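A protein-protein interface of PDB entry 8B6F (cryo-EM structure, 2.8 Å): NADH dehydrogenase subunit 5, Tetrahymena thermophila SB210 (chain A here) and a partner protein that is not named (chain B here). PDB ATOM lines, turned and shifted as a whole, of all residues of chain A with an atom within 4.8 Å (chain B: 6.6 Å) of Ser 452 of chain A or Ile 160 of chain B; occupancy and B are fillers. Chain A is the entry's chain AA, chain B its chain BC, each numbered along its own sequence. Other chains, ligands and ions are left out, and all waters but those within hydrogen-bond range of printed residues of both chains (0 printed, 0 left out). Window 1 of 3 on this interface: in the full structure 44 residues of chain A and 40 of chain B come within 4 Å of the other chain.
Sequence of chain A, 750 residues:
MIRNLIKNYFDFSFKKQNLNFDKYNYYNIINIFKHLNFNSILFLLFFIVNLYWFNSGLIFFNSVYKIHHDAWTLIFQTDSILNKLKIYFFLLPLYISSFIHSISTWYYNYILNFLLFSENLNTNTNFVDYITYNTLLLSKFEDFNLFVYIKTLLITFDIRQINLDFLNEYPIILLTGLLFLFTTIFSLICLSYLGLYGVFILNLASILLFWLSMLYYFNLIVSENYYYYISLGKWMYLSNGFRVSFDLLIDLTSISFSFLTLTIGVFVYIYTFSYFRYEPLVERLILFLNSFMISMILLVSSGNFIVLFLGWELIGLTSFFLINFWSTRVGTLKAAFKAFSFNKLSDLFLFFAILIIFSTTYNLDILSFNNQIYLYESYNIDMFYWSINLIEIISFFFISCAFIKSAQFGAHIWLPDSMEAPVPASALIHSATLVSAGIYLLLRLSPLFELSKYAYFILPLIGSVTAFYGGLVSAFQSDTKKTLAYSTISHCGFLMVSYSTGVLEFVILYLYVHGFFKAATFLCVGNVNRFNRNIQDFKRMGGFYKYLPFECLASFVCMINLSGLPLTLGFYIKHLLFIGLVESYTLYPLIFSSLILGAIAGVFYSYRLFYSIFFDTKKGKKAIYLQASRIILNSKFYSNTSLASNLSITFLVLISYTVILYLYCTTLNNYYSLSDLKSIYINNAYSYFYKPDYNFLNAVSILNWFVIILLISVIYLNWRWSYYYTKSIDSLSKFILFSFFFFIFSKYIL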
ATOM      1  N   GLU A 377      19.895   3.696 -12.650  1.00  0.00           N
ATOM      2  CA  GLU A 377      20.152   4.550 -11.496  1.00  0.00           C
ATOM      3  C   GLU A 377      21.641   4.685 -11.205  1.00  0.00           C
ATOM      4  O   GLU A 377      22.111   5.764 -10.827  1.00  0.00           O
ATOM      5  CB  GLU A 377      19.410   4.001 -10.275  1.00  0.00           C
ATOM      6  CG  GLU A 377      19.730   4.723  -8.973  1.00  0.00           C
ATOM      7  CD  GLU A 377      20.933   4.143  -8.254  1.00  0.00           C
ATOM      8  OE1 GLU A 377      21.215   2.940  -8.432  1.00  0.00           O
ATOM      9  OE2 GLU A 377      21.601   4.893  -7.514  1.00  0.00           O
ATOM     10  N   ILE A 391      20.482  10.101 -12.580  1.00  0.00           N
ATOM     11  CA  ILE A 391      19.198  10.334 -11.930  1.00  0.00           C
ATOM     12  C   ILE A 391      19.138  11.750 -11.379  1.00  0.00           C
ATOM     13  O   ILE A 391      18.119  12.440 -11.504  1.00  0.00           O
ATOM     14  CB  ILE A 391      18.960   9.293 -10.819  1.00  0.00           C
ATOM     15  CG1 ILE A 391      18.987   7.874 -11.388  1.00  0.00           C
ATOM     16  CG2 ILE A 391      17.634   9.558 -10.107  1.00  0.00           C
ATOM     17  CD1 ILE A 391      17.903   7.576 -12.383  1.00  0.00           C
ATOM     18  N   GLU A 392      20.226  12.207 -10.762  1.00  0.00           N
ATOM     19  CA  GLU A 392      20.224  13.531 -10.155  1.00  0.00           C
ATOM     20  C   GLU A 392      20.015  14.622 -11.198  1.00  0.00           C
ATOM     21  O   GLU A 392      19.241  15.559 -10.975  1.00  0.00           O
ATOM     22  CB  GLU A 392      21.534  13.758  -9.402  1.00  0.00           C
ATOM     23  CG  GLU A 392      21.773  12.761  -8.279  1.00  0.00           C
ATOM     24  CD  GLU A 392      20.681  12.774  -7.237  1.00  0.00           C
ATOM     25  OE1 GLU A 392      19.960  13.789  -7.141  1.00  0.00           O
ATOM     26  OE2 GLU A 392      20.539  11.765  -6.516  1.00  0.00           O
ATOM     27  N   SER A 395      16.361  14.401 -12.634  1.00  0.00           N
ATOM     28  CA  SER A 395      15.431  14.896 -11.627  1.00  0.00           C
ATOM     29  C   SER A 395      15.609  16.388 -11.388  1.00  0.00           C
ATOM     30  O   SER A 395      14.637  17.084 -11.076  1.00  0.00           O
ATOM     31  CB  SER A 395      15.614  14.117 -10.327  1.00  0.00           C
ATOM     32  OG  SER A 395      16.964  14.168  -9.898  1.00  0.00           O
ATOM     33  N   LEU A 448      11.330   7.836 -10.570  1.00  0.00           N
ATOM     34  CA  LEU A 448      12.582   8.549 -10.795  1.00  0.00           C
ATOM     35  C   LEU A 448      13.010   9.318  -9.551  1.00  0.00           C
ATOM     36  O   LEU A 448      14.154   9.197  -9.096  1.00  0.00           O
ATOM     37  CB  LEU A 448      12.427   9.498 -11.984  1.00  0.00           C
ATOM     38  CG  LEU A 448      13.600  10.432 -12.289  1.00  0.00           C
ATOM     39  CD1 LEU A 448      14.788   9.656 -12.831  1.00  0.00           C
ATOM     40  CD2 LEU A 448      13.173  11.510 -13.265  1.00  0.00           C
ATOM     41  N   PHE A 449      12.101  10.111  -8.980  1.00  0.00           N
ATOM     42  CA  PHE A 449      12.464  10.989  -7.873  1.00  0.00           C
ATOM     43  C   PHE A 449      12.684  10.232  -6.572  1.00  0.00           C
ATOM     44  O   PHE A 449      13.327  10.767  -5.662  1.00  0.00           O
ATOM     45  CB  PHE A 449      11.386  12.052  -7.676  1.00  0.00           C
ATOM     46  CG  PHE A 449      11.095  12.852  -8.909  1.00  0.00           C
ATOM     47  CD1 PHE A 449      11.964  13.848  -9.322  1.00  0.00           C
ATOM     48  CD2 PHE A 449       9.953  12.613  -9.653  1.00  0.00           C
ATOM     49  CE1 PHE A 449      11.702  14.587 -10.459  1.00  0.00           C
ATOM     50  CE2 PHE A 449       9.683  13.348 -10.790  1.00  0.00           C
ATOM     51  CZ  PHE A 449      10.559  14.336 -11.194  1.00  0.00           C
ATOM     52  N   GLU A 450      12.161   9.011  -6.455  1.00  0.00           N
ATOM     53  CA  GLU A 450      12.406   8.222  -5.254  1.00  0.00           C
ATOM     54  C   GLU A 450      13.884   7.886  -5.104  1.00  0.00           C
ATOM     55  O   GLU A 450      14.365   7.683  -3.984  1.00  0.00           O
ATOM     56  CB  GLU A 450      11.568   6.945  -5.289  1.00  0.00           C
ATOM     57  CG  GLU A 450      10.076   7.197  -5.146  1.00  0.00           C
ATOM     58  CD  GLU A 450       9.239   5.996  -5.537  1.00  0.00           C
ATOM     59  OE1 GLU A 450       9.823   4.954  -5.899  1.00  0.00           O
ATOM     60  OE2 GLU A 450       7.995   6.096  -5.486  1.00  0.00           O
ATOM     61  N   LEU A 451      14.616   7.832  -6.215  1.00  0.00           N
ATOM     62  CA  LEU A 451      16.046   7.553  -6.218  1.00  0.00           C
ATOM     63  C   LEU A 451      16.864   8.811  -6.488  1.00  0.00           C
ATOM     64  O   LEU A 451      17.981   8.734  -7.002  1.00  0.00           O
ATOM     65  CB  LEU A 451      16.376   6.478  -7.250  1.00  0.00           C
ATOM     66  CG  LEU A 451      15.672   5.136  -7.058  1.00  0.00           C
ATOM     67  CD1 LEU A 451      15.812   4.283  -8.304  1.00  0.00           C
ATOM     68  CD2 LEU A 451      16.231   4.410  -5.847  1.00  0.00           C
ATOM     69  N   SER A 452      16.320   9.974  -6.144  1.00  0.00           N
ATOM     70  CA  SER A 452      16.953  11.259  -6.419  1.00  0.00           C
ATOM     71  C   SER A 452      17.367  11.901  -5.102  1.00  0.00           C
ATOM     72  O   SER A 452      16.516  12.250  -4.278  1.00  0.00           O
ATOM     73  CB  SER A 452      15.995  12.168  -7.186  1.00  0.00           C
ATOM     74  OG  SER A 452      16.532  13.469  -7.337  1.00  0.00           O
ATOM     75  N   LYS A 453      18.679  12.051  -4.905  1.00  0.00           N
ATOM     76  CA  LYS A 453      19.172  12.801  -3.755  1.00  0.00           C
ATOM     77  C   LYS A 453      18.755  14.262  -3.840  1.00  0.00           C
ATOM     78  O   LYS A 453      18.381  14.871  -2.831  1.00  0.00           O
ATOM     79  CB  LYS A 453      20.694  12.680  -3.667  1.00  0.00           C
ATOM     80  CG  LYS A 453      21.338  13.467  -2.533  1.00  0.00           C
ATOM     81  CD  LYS A 453      20.936  12.926  -1.171  1.00  0.00           C
ATOM     82  CE  LYS A 453      21.698  13.632  -0.059  1.00  0.00           C
ATOM     83  NZ  LYS A 453      21.385  13.061   1.280  1.00  0.00           N
ATOM     84  N   TYR A 454      18.819  14.844  -5.040  1.00  0.00           N
ATOM     85  CA  TYR A 454      18.440  16.242  -5.200  1.00  0.00           C
ATOM     86  C   TYR A 454      16.975  16.454  -4.850  1.00  0.00           C
ATOM     87  O   TYR A 454      16.626  17.429  -4.174  1.00  0.00           O
ATOM     88  CB  TYR A 454      18.723  16.704  -6.630  1.00  0.00           C
ATOM     89  CG  TYR A 454      18.230  18.102  -6.917  1.00  0.00           C
ATOM     90  CD1 TYR A 454      18.917  19.212  -6.446  1.00  0.00           C
ATOM     91  CD2 TYR A 454      17.078  18.312  -7.660  1.00  0.00           C
ATOM     92  CE1 TYR A 454      18.468  20.491  -6.703  1.00  0.00           C
ATOM     93  CE2 TYR A 454      16.621  19.586  -7.923  1.00  0.00           C
ATOM     94  CZ  TYR A 454      17.319  20.672  -7.442  1.00  0.00           C
ATOM     95  OH  TYR A 454      16.865  21.941  -7.707  1.00  0.00           O
ATOM     96  N   ALA A 455      16.102  15.546  -5.287  1.00  0.00           N
ATOM     97  CA  ALA A 455      14.688  15.660  -4.952  1.00  0.00           C
ATOM     98  C   ALA A 455      14.486  15.614  -3.444  1.00  0.00           C
ATOM     99  O   ALA A 455      13.724  16.406  -2.879  1.00  0.00           O
ATOM    100  CB  ALA A 455      13.896  14.544  -5.632  1.00  0.00           C
ATOM    101  N   TYR A 456      15.154  14.673  -2.779  1.00  0.00           N
ATOM    102  CA  TYR A 456      15.002  14.524  -1.336  1.00  0.00           C
ATOM    103  C   TYR A 456      15.342  15.816  -0.606  1.00  0.00           C
ATOM    104  O   TYR A 456      14.628  16.221   0.318  1.00  0.00           O
ATOM    105  CB  TYR A 456      15.890  13.376  -0.852  1.00  0.00           C
ATOM    106  CG  TYR A 456      16.074  13.301   0.646  1.00  0.00           C
ATOM    107  CD1 TYR A 456      15.208  12.555   1.433  1.00  0.00           C
ATOM    108  CD2 TYR A 456      17.132  13.950   1.270  1.00  0.00           C
ATOM    109  CE1 TYR A 456      15.378  12.471   2.799  1.00  0.00           C
ATOM    110  CE2 TYR A 456      17.311  13.872   2.637  1.00  0.00           C
ATOM    111  CZ  TYR A 456      16.432  13.131   3.395  1.00  0.00           C
ATOM    112  OH  TYR A 456      16.604  13.050   4.756  1.00  0.00           O
ATOM    113  N   PHE B 120      12.277  -1.886  -2.496  1.00  0.00           N
ATOM    114  CA  PHE B 120      12.966  -0.640  -2.811  1.00  0.00           C
ATOM    115  C   PHE B 120      14.379  -0.636  -2.239  1.00  0.00           C
ATOM    116  O   PHE B 120      15.346  -0.323  -2.942  1.00  0.00           O
ATOM    117  CB  PHE B 120      12.165   0.547  -2.275  1.00  0.00           C
ATOM    118  CG  PHE B 120      12.835   1.870  -2.487  1.00  0.00           C
ATOM    119  CD1 PHE B 120      12.713   2.536  -3.693  1.00  0.00           C
ATOM    120  CD2 PHE B 120      13.587   2.449  -1.480  1.00  0.00           C
ATOM    121  CE1 PHE B 120      13.329   3.754  -3.893  1.00  0.00           C
ATOM    122  CE2 PHE B 120      14.206   3.668  -1.673  1.00  0.00           C
ATOM    123  CZ  PHE B 120      14.077   4.321  -2.881  1.00  0.00           C
ATOM    124  N   TYR B 124      17.890  -1.650  -4.541  1.00  0.00           N
ATOM    125  CA  TYR B 124      18.959  -0.663  -4.629  1.00  0.00           C
ATOM    126  C   TYR B 124      20.323  -1.320  -4.465  1.00  0.00           C
ATOM    127  O   TYR B 124      21.237  -1.091  -5.264  1.00  0.00           O
ATOM    128  CB  TYR B 124      18.758   0.427  -3.578  1.00  0.00           C
ATOM    129  CG  TYR B 124      19.792   1.523  -3.655  1.00  0.00           C
ATOM    130  CD1 TYR B 124      19.613   2.615  -4.493  1.00  0.00           C
ATOM    131  CD2 TYR B 124      20.951   1.462  -2.896  1.00  0.00           C
ATOM    132  CE1 TYR B 124      20.557   3.615  -4.571  1.00  0.00           C
ATOM    133  CE2 TYR B 124      21.902   2.458  -2.965  1.00  0.00           C
ATOM    134  CZ  TYR B 124      21.699   3.533  -3.803  1.00  0.00           C
ATOM    135  OH  TYR B 124      22.645   4.526  -3.876  1.00  0.00           O
ATOM    136  N   TYR B 128      23.793  -2.874  -7.390  1.00  0.00           N
ATOM    137  CA  TYR B 128      25.234  -2.739  -7.217  1.00  0.00           C
ATOM    138  C   TYR B 128      25.908  -4.090  -7.015  1.00  0.00           C
ATOM    139  O   TYR B 128      27.079  -4.254  -7.373  1.00  0.00           O
ATOM    140  CB  TYR B 128      25.536  -1.816  -6.039  1.00  0.00           C
ATOM    141  CG  TYR B 128      25.182  -0.373  -6.301  1.00  0.00           C
ATOM    142  CD1 TYR B 128      26.075   0.477  -6.938  1.00  0.00           C
ATOM    143  CD2 TYR B 128      23.955   0.140  -5.909  1.00  0.00           C
ATOM    144  CE1 TYR B 128      25.756   1.797  -7.180  1.00  0.00           C
ATOM    145  CE2 TYR B 128      23.626   1.456  -6.145  1.00  0.00           C
ATOM    146  CZ  TYR B 128      24.529   2.280  -6.781  1.00  0.00           C
ATOM    147  OH  TYR B 128      24.201   3.594  -7.016  1.00  0.00           O
ATOM    148  N   ASN B 158      28.070   7.862  -3.345  1.00  0.00           N
ATOM    149  CA  ASN B 158      27.465   9.166  -3.111  1.00  0.00           C
ATOM    150  C   ASN B 158      26.074   9.216  -3.729  1.00  0.00           C
ATOM    151  O   ASN B 158      25.645   8.301  -4.436  1.00  0.00           O
ATOM    152  CB  ASN B 158      28.336  10.292  -3.681  1.00  0.00           C
ATOM    153  CG  ASN B 158      28.372  10.293  -5.194  1.00  0.00           C
ATOM    154  OD1 ASN B 158      27.444  10.768  -5.847  1.00  0.00           O
ATOM    155  ND2 ASN B 158      29.449   9.767  -5.761  1.00  0.00           N
ATOM    156  N   GLY B 159      25.370  10.305  -3.450  1.00  0.00           N
ATOM    157  CA  GLY B 159      24.025  10.490  -3.970  1.00  0.00           C
ATOM    158  C   GLY B 159      22.986  10.029  -2.969  1.00  0.00           C
ATOM    159  O   GLY B 159      23.026  10.420  -1.804  1.00  0.00           O
ATOM    160  N   ILE B 160      22.049   9.193  -3.428  1.00  0.00           N
ATOM    161  CA  ILE B 160      21.009   8.659  -2.551  1.00  0.00           C
ATOM    162  C   ILE B 160      21.525   7.548  -1.655  1.00  0.00           C
ATOM    163  O   ILE B 160      20.761   7.020  -0.838  1.00  0.00           O
ATOM    164  CB  ILE B 160      19.817   8.160  -3.397  1.00  0.00           C
ATOM    165  CG1 ILE B 160      18.530   8.102  -2.564  1.00  0.00           C
ATOM    166  CG2 ILE B 160      20.102   6.794  -4.009  1.00  0.00           C
ATOM    167  CD1 ILE B 160      17.977   9.460  -2.181  1.00  0.00           C
ATOM    168  N   ARG B 161      22.805   7.189  -1.766  1.00  0.00           N
ATOM    169  CA  ARG B 161      23.356   6.135  -0.921  1.00  0.00           C
ATOM    170  C   ARG B 161      23.191   6.473   0.555  1.00  0.00           C
ATOM    171  O   ARG B 161      22.828   5.610   1.360  1.00  0.00           O
ATOM    172  CB  ARG B 161      24.831   5.919  -1.262  1.00  0.00           C
ATOM    173  CG  ARG B 161      25.556   4.919  -0.372  1.00  0.00           C
ATOM    174  CD  ARG B 161      25.202   3.488  -0.723  1.00  0.00           C
ATOM    175  NE  ARG B 161      25.852   3.064  -1.957  1.00  0.00           N
ATOM    176  CZ  ARG B 161      25.948   1.805  -2.361  1.00  0.00           C
ATOM    177  NH1 ARG B 161      25.449   0.810  -1.649  1.00  0.00           N
ATOM    178  NH2 ARG B 161      26.567   1.539  -3.508  1.00  0.00           N
ATOM    179  N   ASP B 162      23.454   7.726   0.929  1.00  0.00           N
ATOM    180  CA  ASP B 162      23.334   8.111   2.331  1.00  0.00           C
ATOM    181  C   ASP B 162      21.899   7.972   2.820  1.00  0.00           C
ATOM    182  O   ASP B 162      21.659   7.485   3.930  1.00  0.00           O
ATOM    183  CB  ASP B 162      23.830   9.544   2.521  1.00  0.00           C
ATOM    184  CG  ASP B 162      25.308   9.690   2.228  1.00  0.00           C
ATOM    185  OD1 ASP B 162      26.074   8.764   2.567  1.00  0.00           O
ATOM    186  OD2 ASP B 162      25.705  10.726   1.656  1.00  0.00           O
ATOM    187  N   VAL B 163      20.930   8.403   2.011  1.00  0.00           N
ATOM    188  CA  VAL B 163      19.531   8.286   2.409  1.00  0.00           C
ATOM    189  C   VAL B 163      19.141   6.823   2.559  1.00  0.00           C
ATOM    190  O   VAL B 163      18.464   6.439   3.520  1.00  0.00           O
ATOM    191  CB  VAL B 163      18.626   9.013   1.397  1.00  0.00           C
ATOM    192  CG1 VAL B 163      17.159   8.844   1.764  1.00  0.00           C
ATOM    193  CG2 VAL B 163      18.991  10.487   1.324  1.00  0.00           C
ATOM    194  N   ILE B 164      19.559   5.980   1.613  1.00  0.00           N
ATOM    195  CA  ILE B 164      19.223   4.561   1.685  1.00  0.00           C
ATOM    196  C   ILE B 164      19.843   3.935   2.927  1.00  0.00           C
ATOM    197  O   ILE B 164      19.200   3.145   3.629  1.00  0.00           O
ATOM    198  CB  ILE B 164      19.673   3.839   0.401  1.00  0.00           C
ATOM    199  CG1 ILE B 164      18.940   4.398  -0.823  1.00  0.00           C
ATOM    200  CG2 ILE B 164      19.444   2.333   0.519  1.00  0.00           C
ATOM    201  CD1 ILE B 164      17.441   4.178  -0.827  1.00  0.00           C
ATOM    202  N   ASP B 165      21.102   4.272   3.216  1.00  0.00           N
ATOM    203  CA  ASP B 165      21.753   3.726   4.402  1.00  0.00           C
ATOM    204  C   ASP B 165      21.047   4.174   5.674  1.00  0.00           C
ATOM    205  O   ASP B 165      20.856   3.377   6.598  1.00  0.00           O
ATOM    206  CB  ASP B 165      23.221   4.147   4.433  1.00  0.00           C
ATOM    207  CG  ASP B 165      24.030   3.518   3.320  1.00  0.00           C
ATOM    208  OD1 ASP B 165      23.476   2.676   2.584  1.00  0.00           O
ATOM    209  OD2 ASP B 165      25.223   3.863   3.179  1.00  0.00           O
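The side-chain carboxylate (OE1) of Glu 392 of chain A sits at hydrogen-bond distance from the side-chain hydroxyl (OG) of Ser 452 of chain A, at 3.4 Å. The side-chain carboxylate (OE2) of Glu 392 of chain A sits at hydrogen-bond distance from the backbone NH (N) of Lys 453 of chain A, at 2.5 Å. The side-chain hydroxyl of Ser 452 of chain A sits at hydrogen-bond distance from the side-chain hydroxyl of Ser 395 of chain A. The side-chain hydroxyl (OG) of Ser 452 of chain A lies within hydrogen-bond range of the backbone NH (N) of Ala 455 of chain A (2.9 Å). The backbone NH (N) of Arg 161 of chain B sits at hydrogen-bond distance from the side-chain hydroxyl (OH) of Tyr 124 of chain B, at 3.4 Å.
Of the 11 printed residues of chain B, 6 touch a printed residue of chain A. Hydrophobic or aromatic side chains of chain B within 4 Å of the printed part of chain A: Phe 120, Tyr 124, Tyr 128, Ile 160 and Val 163. Hydrophobic or aromatic side chains of chain A within 4 Å of the printed part of chain B: Leu 451 and Tyr 456.
Ile 160 of chain B touches two residues of chain A. Of the printed residues of chain A, Gly 159 of chain B touches Lys 453. Of the printed residues of chain A, Phe 120 of chain B touches Glu 450 and Leu 451. Of the printed residues of chain B, Leu 451 of chain A touches Phe 120. Asp 162 of chain B touches none of the printed residues of chain A. Glu 392 of chain A touches none of the printed residues of chain B. The nearest printed residue of chain A that does not touch Tyr 124 of chain B is Leu 451 of chain A (4.1 Å).
Among the printed residues, merely in contact across the chains: Glu 377 of chain A with Tyr 124 of chain B (3.4 Å), Glu 450 of chain A with Phe 120 of chain B (3.6 Å), Leu 451 of chain A with Phe 120 of chain B (3.6 Å), Ser 452 of chain A with Ile 160 of chain B (3.8 Å), Lys 453 of chain A with Gly 159 of chain B (3.3 Å), Lys 453 of chain A with Ile 160 of chain B (3.7 Å), Lys 453 of chain A with Val 163 of chain B (3.5 Å) and Tyr 456 of chain A with Val 163 of chain B (3.9 Å).
The side-chain hydroxyl of Tyr 128 of chain B lies within hydrogen-bond range of the side-chain carboxylate of Glu 377 of chain A (2.9 Å).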
